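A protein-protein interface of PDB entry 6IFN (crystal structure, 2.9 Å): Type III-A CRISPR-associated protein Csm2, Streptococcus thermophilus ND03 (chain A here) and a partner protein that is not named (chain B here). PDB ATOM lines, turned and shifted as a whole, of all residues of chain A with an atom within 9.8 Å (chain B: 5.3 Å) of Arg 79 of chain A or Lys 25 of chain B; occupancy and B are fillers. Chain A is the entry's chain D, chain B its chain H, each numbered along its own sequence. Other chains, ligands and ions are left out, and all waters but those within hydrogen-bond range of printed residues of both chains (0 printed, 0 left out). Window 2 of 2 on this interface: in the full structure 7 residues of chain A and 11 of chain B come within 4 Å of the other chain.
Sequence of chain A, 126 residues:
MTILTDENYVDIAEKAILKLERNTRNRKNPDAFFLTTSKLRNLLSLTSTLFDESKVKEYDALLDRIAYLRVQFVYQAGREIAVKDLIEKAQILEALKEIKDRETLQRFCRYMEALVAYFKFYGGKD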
ATOM      1  N   LYS A  39     -20.206 -10.259  31.869  1.00  0.00           N
ATOM      2  CA  LYS A  39     -18.955 -10.888  31.404  1.00  0.00           C
ATOM      3  C   LYS A  39     -19.021 -11.077  29.881  1.00  0.00           C
ATOM      4  O   LYS A  39     -18.055 -10.796  29.163  1.00  0.00           O
ATOM      5  CB  LYS A  39     -18.692 -12.211  32.136  1.00  0.00           C
ATOM      6  N   LEU A  43     -18.797  -9.504  23.532  1.00  0.00           N
ATOM      7  CA  LEU A  43     -18.750 -10.454  22.439  1.00  0.00           C
ATOM      8  C   LEU A  43     -20.171 -10.728  21.919  1.00  0.00           C
ATOM      9  O   LEU A  43     -20.309 -11.103  20.785  1.00  0.00           O
ATOM     10  CB  LEU A  43     -17.954 -11.725  22.782  1.00  0.00           C
ATOM     11  CG  LEU A  43     -18.084 -12.345  24.173  1.00  0.00           C
ATOM     12  CD1 LEU A  43     -19.475 -12.906  24.391  1.00  0.00           C
ATOM     13  CD2 LEU A  43     -17.059 -13.454  24.353  1.00  0.00           C
ATOM     14  N   VAL A  71     -11.052 -14.192  18.615  1.00  0.00           N
ATOM     15  CA  VAL A  71     -10.024 -13.581  19.445  1.00  0.00           C
ATOM     16  C   VAL A  71     -10.638 -13.241  20.807  1.00  0.00           C
ATOM     17  O   VAL A  71     -10.201 -13.782  21.835  1.00  0.00           O
ATOM     18  CB  VAL A  71      -9.399 -12.341  18.769  1.00  0.00           C
ATOM     19  CG1 VAL A  71      -8.754 -11.387  19.765  1.00  0.00           C
ATOM     20  CG2 VAL A  71      -8.383 -12.727  17.714  1.00  0.00           C
ATOM     21  N   GLN A  72     -11.630 -12.338  20.804  1.00  0.00           N
ATOM     22  CA  GLN A  72     -12.228 -11.864  22.046  1.00  0.00           C
ATOM     23  C   GLN A  72     -12.850 -13.045  22.800  1.00  0.00           C
ATOM     24  O   GLN A  72     -12.892 -13.029  24.018  1.00  0.00           O
ATOM     25  CB  GLN A  72     -13.210 -10.716  21.816  1.00  0.00           C
ATOM     26  CG  GLN A  72     -12.602  -9.359  22.126  1.00  0.00           C
ATOM     27  CD  GLN A  72     -11.533  -8.991  21.125  1.00  0.00           C
ATOM     28  OE1 GLN A  72     -11.318  -9.668  20.120  1.00  0.00           O
ATOM     29  NE2 GLN A  72     -10.866  -7.880  21.381  1.00  0.00           N
ATOM     30  N   PHE A  73     -13.305 -14.081  22.097  1.00  0.00           N
ATOM     31  CA  PHE A  73     -13.762 -15.296  22.775  1.00  0.00           C
ATOM     32  C   PHE A  73     -12.627 -15.825  23.659  1.00  0.00           C
ATOM     33  O   PHE A  73     -12.808 -16.027  24.846  1.00  0.00           O
ATOM     34  CB  PHE A  73     -14.285 -16.343  21.784  1.00  0.00           C
ATOM     35  CG  PHE A  73     -15.773 -16.253  21.541  1.00  0.00           C
ATOM     36  CD1 PHE A  73     -16.664 -16.740  22.485  1.00  0.00           C
ATOM     37  CD2 PHE A  73     -16.287 -15.638  20.402  1.00  0.00           C
ATOM     38  CE1 PHE A  73     -18.030 -16.645  22.280  1.00  0.00           C
ATOM     39  CE2 PHE A  73     -17.653 -15.525  20.204  1.00  0.00           C
ATOM     40  CZ  PHE A  73     -18.520 -16.040  21.141  1.00  0.00           C
ATOM     41  N   VAL A  74     -11.451 -16.032  23.067  1.00  0.00           N
ATOM     42  CA  VAL A  74     -10.320 -16.616  23.784  1.00  0.00           C
ATOM     43  C   VAL A  74      -9.868 -15.643  24.889  1.00  0.00           C
ATOM     44  O   VAL A  74      -9.712 -16.043  26.040  1.00  0.00           O
ATOM     45  CB  VAL A  74      -9.174 -16.998  22.823  1.00  0.00           C
ATOM     46  CG1 VAL A  74      -8.145 -17.863  23.527  1.00  0.00           C
ATOM     47  CG2 VAL A  74      -9.670 -17.697  21.560  1.00  0.00           C
ATOM     48  N   TYR A  75      -9.664 -14.365  24.538  1.00  0.00           N
ATOM     49  CA  TYR A  75      -9.222 -13.337  25.490  1.00  0.00           C
ATOM     50  C   TYR A  75     -10.109 -13.376  26.737  1.00  0.00           C
ATOM     51  O   TYR A  75      -9.625 -13.528  27.856  1.00  0.00           O
ATOM     52  CB  TYR A  75      -9.275 -11.964  24.820  1.00  0.00           C
ATOM     53  CG  TYR A  75      -8.686 -10.798  25.576  1.00  0.00           C
ATOM     54  CD1 TYR A  75      -9.180 -10.367  26.801  1.00  0.00           C
ATOM     55  CD2 TYR A  75      -7.691 -10.032  24.985  1.00  0.00           C
ATOM     56  CE1 TYR A  75      -8.644  -9.259  27.448  1.00  0.00           C
ATOM     57  CE2 TYR A  75      -7.154  -8.915  25.609  1.00  0.00           C
ATOM     58  CZ  TYR A  75      -7.630  -8.523  26.846  1.00  0.00           C
ATOM     59  OH  TYR A  75      -7.061  -7.419  27.419  1.00  0.00           O
ATOM     60  N   GLN A  76     -11.423 -13.254  26.515  1.00  0.00           N
ATOM     61  CA  GLN A  76     -12.398 -13.257  27.595  1.00  0.00           C
ATOM     62  C   GLN A  76     -12.421 -14.616  28.286  1.00  0.00           C
ATOM     63  O   GLN A  76     -12.746 -14.672  29.453  1.00  0.00           O
ATOM     64  CB  GLN A  76     -13.798 -12.899  27.089  1.00  0.00           C
ATOM     65  CG  GLN A  76     -13.943 -11.405  26.824  1.00  0.00           C
ATOM     66  CD  GLN A  76     -13.641 -10.632  28.081  1.00  0.00           C
ATOM     67  OE1 GLN A  76     -13.930 -11.102  29.179  1.00  0.00           O
ATOM     68  NE2 GLN A  76     -13.025  -9.468  27.929  1.00  0.00           N
ATOM     69  N   ALA A  77     -12.129 -15.690  27.549  1.00  0.00           N
ATOM     70  CA  ALA A  77     -12.033 -17.021  28.119  1.00  0.00           C
ATOM     71  C   ALA A  77     -10.909 -17.034  29.157  1.00  0.00           C
ATOM     72  O   ALA A  77     -11.032 -17.671  30.207  1.00  0.00           O
ATOM     73  CB  ALA A  77     -11.802 -18.047  27.036  1.00  0.00           C
ATOM     74  N   GLY A  78      -9.825 -16.313  28.858  1.00  0.00           N
ATOM     75  CA  GLY A  78      -8.728 -16.148  29.793  1.00  0.00           C
ATOM     76  C   GLY A  78      -9.121 -15.295  30.992  1.00  0.00           C
ATOM     77  O   GLY A  78      -8.855 -15.649  32.157  1.00  0.00           O
ATOM     78  N   ARG A  79      -9.778 -14.168  30.716  1.00  0.00           N
ATOM     79  CA  ARG A  79      -9.965 -13.112  31.707  1.00  0.00           C
ATOM     80  C   ARG A  79     -10.941 -13.526  32.823  1.00  0.00           C
ATOM     81  O   ARG A  79     -10.883 -12.958  33.909  1.00  0.00           O
ATOM     82  CB  ARG A  79     -10.442 -11.833  31.015  1.00  0.00           C
ATOM     83  CG  ARG A  79      -9.339 -11.059  30.307  1.00  0.00           C
ATOM     84  CD  ARG A  79      -9.242  -9.615  30.775  1.00  0.00           C
ATOM     85  NE  ARG A  79      -9.305  -9.517  32.230  1.00  0.00           N
ATOM     86  CZ  ARG A  79      -9.725  -8.442  32.890  1.00  0.00           C
ATOM     87  NH1 ARG A  79      -9.845  -7.290  32.249  1.00  0.00           N
ATOM     88  NH2 ARG A  79     -10.046  -8.524  34.171  1.00  0.00           N
ATOM     89  N   GLU A  80     -11.828 -14.498  32.553  1.00  0.00           N
ATOM     90  CA  GLU A  80     -12.836 -14.969  33.520  1.00  0.00           C
ATOM     91  C   GLU A  80     -13.038 -16.479  33.295  1.00  0.00           C
ATOM     92  O   GLU A  80     -13.016 -16.967  32.171  1.00  0.00           O
ATOM     93  CB  GLU A  80     -14.167 -14.216  33.366  1.00  0.00           C
ATOM     94  CG  GLU A  80     -14.053 -12.702  33.147  1.00  0.00           C
ATOM     95  CD  GLU A  80     -13.867 -11.818  34.377  1.00  0.00           C
ATOM     96  OE1 GLU A  80     -13.498 -10.636  34.195  1.00  0.00           O
ATOM     97  OE2 GLU A  80     -14.123 -12.288  35.513  1.00  0.00           O
ATOM     98  N   ILE A  81     -13.255 -17.227  34.377  1.00  0.00           N
ATOM     99  CA  ILE A  81     -13.231 -18.687  34.337  1.00  0.00           C
ATOM    100  C   ILE A  81     -14.573 -19.209  33.792  1.00  0.00           C
ATOM    101  O   ILE A  81     -14.576 -20.149  32.991  1.00  0.00           O
ATOM    102  CB  ILE A  81     -12.849 -19.267  35.719  1.00  0.00           C
ATOM    103  CG1 ILE A  81     -11.463 -18.770  36.159  1.00  0.00           C
ATOM    104  CG2 ILE A  81     -12.912 -20.791  35.736  1.00  0.00           C
ATOM    105  CD1 ILE A  81     -11.439 -17.448  36.924  1.00  0.00           C
ATOM    106  N   ALA A  82     -15.689 -18.607  34.228  1.00  0.00           N
ATOM    107  CA  ALA A  82     -17.060 -19.083  33.888  1.00  0.00           C
ATOM    108  C   ALA A  82     -17.346 -18.916  32.388  1.00  0.00           C
ATOM    109  O   ALA A  82     -18.091 -19.714  31.848  1.00  0.00           O
ATOM    110  CB  ALA A  82     -18.110 -18.381  34.719  1.00  0.00           C
ATOM    111  N   VAL A  83     -16.766 -17.888  31.750  1.00  0.00           N
ATOM    112  CA  VAL A  83     -16.831 -17.732  30.291  1.00  0.00           C
ATOM    113  C   VAL A  83     -16.157 -18.935  29.612  1.00  0.00           C
ATOM    114  O   VAL A  83     -16.784 -19.598  28.790  1.00  0.00           O
ATOM    115  CB  VAL A  83     -16.235 -16.398  29.800  1.00  0.00           C
ATOM    116  CG1 VAL A  83     -15.716 -16.475  28.373  1.00  0.00           C
ATOM    117  CG2 VAL A  83     -17.257 -15.273  29.905  1.00  0.00           C
ATOM    118  N   LYS A  84     -14.897 -19.216  29.960  1.00  0.00           N
ATOM    119  CA  LYS A  84     -14.161 -20.343  29.344  1.00  0.00           C
ATOM    120  C   LYS A  84     -14.997 -21.618  29.523  1.00  0.00           C
ATOM    121  O   LYS A  84     -15.118 -22.415  28.587  1.00  0.00           O
ATOM    122  CB  LYS A  84     -12.749 -20.503  29.926  1.00  0.00           C
ATOM    123  N   ASP A  85     -15.580 -21.777  30.719  1.00  0.00           N
ATOM    124  CA  ASP A  85     -16.426 -22.918  31.033  1.00  0.00           C
ATOM    125  C   ASP A  85     -17.604 -22.997  30.044  1.00  0.00           C
ATOM    126  O   ASP A  85     -17.901 -24.066  29.493  1.00  0.00           O
ATOM    127  CB  ASP A  85     -16.920 -22.854  32.478  1.00  0.00           C
ATOM    128  CG  ASP A  85     -17.920 -23.942  32.829  1.00  0.00           C
ATOM    129  OD1 ASP A  85     -17.920 -24.995  32.155  1.00  0.00           O
ATOM    130  OD2 ASP A  85     -18.697 -23.731  33.774  1.00  0.00           O
ATOM    131  N   ILE A  87     -17.878 -21.600  27.014  1.00  0.00           N
ATOM    132  CA  ILE A  87     -17.351 -21.913  25.687  1.00  0.00           C
ATOM    133  C   ILE A  87     -17.053 -23.417  25.555  1.00  0.00           C
ATOM    134  O   ILE A  87     -17.129 -23.981  24.461  1.00  0.00           O
ATOM    135  CB  ILE A  87     -16.106 -21.065  25.376  1.00  0.00           C
ATOM    136  CG1 ILE A  87     -16.343 -19.600  25.741  1.00  0.00           C
ATOM    137  CG2 ILE A  87     -15.685 -21.233  23.922  1.00  0.00           C
ATOM    138  CD1 ILE A  87     -15.321 -18.657  25.170  1.00  0.00           C
ATOM    139  N   GLY B  23     -15.180   0.726  31.553  1.00  0.00           N
ATOM    140  CA  GLY B  23     -15.231  -0.473  32.387  1.00  0.00           C
ATOM    141  C   GLY B  23     -14.103  -1.459  32.114  1.00  0.00           C
ATOM    142  O   GLY B  23     -13.791  -2.295  32.957  1.00  0.00           O
ATOM    143  N   GLU B  24     -13.501  -1.384  30.924  1.00  0.00           N
ATOM    144  CA  GLU B  24     -12.597  -2.433  30.434  1.00  0.00           C
ATOM    145  C   GLU B  24     -11.194  -2.213  31.010  1.00  0.00           C
ATOM    146  O   GLU B  24     -10.852  -1.100  31.429  1.00  0.00           O
ATOM    147  CB  GLU B  24     -12.601  -2.445  28.917  1.00  0.00           C
ATOM    148  N   LYS B  25     -10.379  -3.271  31.022  1.00  0.00           N
ATOM    149  CA  LYS B  25      -9.006  -3.152  31.494  1.00  0.00           C
ATOM    150  C   LYS B  25      -8.098  -4.133  30.748  1.00  0.00           C
ATOM    151  O   LYS B  25      -8.402  -5.335  30.696  1.00  0.00           O
ATOM    152  CB  LYS B  25      -8.934  -3.378  33.010  1.00  0.00           C
ATOM    153  CG  LYS B  25      -9.942  -4.342  33.631  1.00  0.00           C
ATOM    154  CD  LYS B  25      -9.474  -4.880  34.986  1.00  0.00           C
ATOM    155  CE  LYS B  25      -9.681  -3.905  36.126  1.00  0.00           C
ATOM    156  NZ  LYS B  25     -11.064  -3.977  36.641  1.00  0.00           N
ATOM    157  N   TYR B  26      -6.982  -3.600  30.209  1.00  0.00           N
ATOM    158  CA  TYR B  26      -5.918  -4.387  29.534  1.00  0.00           C
ATOM    159  C   TYR B  26      -5.265  -5.370  30.504  1.00  0.00           C
ATOM    160  O   TYR B  26      -4.984  -5.017  31.645  1.00  0.00           O
ATOM    161  CB  TYR B  26      -4.749  -3.531  29.067  1.00  0.00           C
ATOM    162  CG  TYR B  26      -5.074  -2.360  28.185  1.00  0.00           C
ATOM    163  CD1 TYR B  26      -5.481  -2.532  26.878  1.00  0.00           C
ATOM    164  CD2 TYR B  26      -4.872  -1.066  28.632  1.00  0.00           C
ATOM    165  CE1 TYR B  26      -5.713  -1.446  26.045  1.00  0.00           C
ATOM    166  CE2 TYR B  26      -5.106   0.033  27.815  1.00  0.00           C
ATOM    167  CZ  TYR B  26      -5.519  -0.154  26.509  1.00  0.00           C
ATOM    168  OH  TYR B  26      -5.719   0.939  25.709  1.00  0.00           O
ATOM    169  N   THR B  27      -4.986  -6.578  30.015  1.00  0.00           N
ATOM    170  CA  THR B  27      -4.336  -7.610  30.791  1.00  0.00           C
ATOM    171  C   THR B  27      -2.902  -7.802  30.274  1.00  0.00           C
ATOM    172  O   THR B  27      -2.617  -7.511  29.097  1.00  0.00           O
ATOM    173  CB  THR B  27      -5.136  -8.910  30.718  1.00  0.00           C
ATOM    174  OG1 THR B  27      -4.759  -9.764  31.797  1.00  0.00           O
ATOM    175  CG2 THR B  27      -4.917  -9.646  29.418  1.00  0.00           C
ATOM    176  N   THR B  66      -5.180 -19.073  30.351  1.00  0.00           N
ATOM    177  CA  THR B  66      -5.363 -18.406  31.610  1.00  0.00           C
ATOM    178  C   THR B  66      -6.292 -19.260  32.484  1.00  0.00           C
ATOM    179  O   THR B  66      -7.510 -19.167  32.426  1.00  0.00           O
ATOM    180  CB  THR B  66      -5.872 -16.997  31.421  1.00  0.00           C
ATOM    181  N   GLU B 113      -1.720  -5.745  35.095  1.00  0.00           N
ATOM    182  CA  GLU B 113      -3.106  -5.313  34.839  1.00  0.00           C
ATOM    183  C   GLU B 113      -3.209  -3.777  34.849  1.00  0.00           C
ATOM    184  O   GLU B 113      -2.678  -3.097  35.735  1.00  0.00           O
ATOM    185  CB  GLU B 113      -4.021  -5.919  35.904  1.00  0.00           C
ATOM    186  CG  GLU B 113      -5.467  -6.066  35.479  1.00  0.00           C
ATOM    187  CD  GLU B 113      -6.314  -6.596  36.617  1.00  0.00           C
ATOM    188  OE1 GLU B 113      -6.455  -5.879  37.615  1.00  0.00           O
ATOM    189  OE2 GLU B 113      -6.786  -7.734  36.520  1.00  0.00           O
ATOM    190  N   VAL B 114      -3.938  -3.237  33.870  1.00  0.00           N
ATOM    191  CA  VAL B 114      -4.046  -1.796  33.628  1.00  0.00           C
ATOM    192  C   VAL B 114      -5.503  -1.442  33.292  1.00  0.00           C
ATOM    193  O   VAL B 114      -6.182  -2.205  32.600  1.00  0.00           O
ATOM    194  CB  VAL B 114      -3.103  -1.375  32.484  1.00  0.00           C
ATOM    195  CG1 VAL B 114      -3.221   0.111  32.148  1.00  0.00           C
ATOM    196  CG2 VAL B 114      -1.672  -1.772  32.783  1.00  0.00           C
ATOM    197  N   ASN B 115      -5.947  -0.255  33.728  1.00  0.00           N
ATOM    198  CA  ASN B 115      -7.315   0.213  33.512  1.00  0.00           C
ATOM    199  C   ASN B 115      -7.356   1.177  32.319  1.00  0.00           C
ATOM    200  O   ASN B 115      -6.708   2.220  32.345  1.00  0.00           O
ATOM    201  CB  ASN B 115      -7.888   0.850  34.777  1.00  0.00           C
ATOM    202  CG  ASN B 115      -8.300  -0.184  35.799  1.00  0.00           C
ATOM    203  OD1 ASN B 115      -8.044  -1.368  35.608  1.00  0.00           O
ATOM    204  ND2 ASN B 115      -8.901   0.251  36.895  1.00  0.00           N
ATOM    205  N   LYS B 116      -8.141   0.808  31.293  1.00  0.00           N
ATOM    206  CA  LYS B 116      -8.270   1.584  30.053  1.00  0.00           C
ATOM    207  C   LYS B 116      -8.911   2.933  30.364  1.00  0.00           C
ATOM    208  O   LYS B 116      -9.868   3.001  31.159  1.00  0.00           O
ATOM    209  CB  LYS B 116      -9.195   0.883  29.053  1.00  0.00           C
ATOM    210  CG  LYS B 116      -8.608  -0.277  28.258  1.00  0.00           C
ATOM    211  CD  LYS B 116      -9.668  -1.074  27.514  1.00  0.00           C
ATOM    212  CE  LYS B 116      -9.219  -1.567  26.156  1.00  0.00           C
ATOM    213  NZ  LYS B 116      -9.241  -0.491  25.136  1.00  0.00           N
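Printed residues of chain B within 4 Å of Tyr 75 of chain A: Tyr 26 (3.9 Å) and Thr 27 (3.4 Å). Of the printed residues of chain B, Gly 78 of chain A touches Thr 66. Of chain B, only Lys 25 comes within 4 Å of Arg 79 of chain A. No residue of chain A comes within 4 Å of Glu 24 of chain B. Lys 25 of chain B touches one residue of chain A. Printed residues of chain A within 4 Å of Tyr 26 of chain B: Tyr 75 (3.9 Å). Of the printed residues of chain A, Thr 66 of chain B touches Gly 78 (3.4 Å). Asn 115 of chain B touches none of the printed residues of chain A. The nearest residue of chain B that does not touch Arg 79 of chain A is Glu 113 of chain B (4.1 Å). The nearest residue of chain A that does not touch Lys 25 of chain B is Tyr 75 of chain A (4.1 Å).
Among the printed residues, pairs that only touch across the chains: Gly 78 of chain A with Thr 66 of chain B (3.4 Å) and Tyr 75 of chain A with Tyr 26 of chain B (3.9 Å).
Printed residues of chain B that touch a printed residue of chain A: Lys 25, Tyr 26, Thr 27 and Thr 66. Printed residues of chain A that touch a printed residue of chain B: Tyr 75, Gly 78 and Arg 79. Hydrophobic or aromatic side chains of chain A within 4 Å of the printed part of chain B: Tyr 75. Among the printed residues, 4 pairs touch across the chains. Among the printed residues, no Asp or Glu carboxylate lies within 4 Å of a Lys or Arg side-chain nitrogen of the other chain.
OH of Tyr 75 of chain A lies within hydrogen-bond range of N of Thr 27 of chain B. The guanidinium group of Arg 79 of chain A is in hydrogen-bond range of the backbone carbonyl oxygen of Lys 25 of chain B (2.9 Å).
O of Val 114 of chain B is in hydrogen-bond range of N of Tyr 26 of chain B (2.9 Å).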
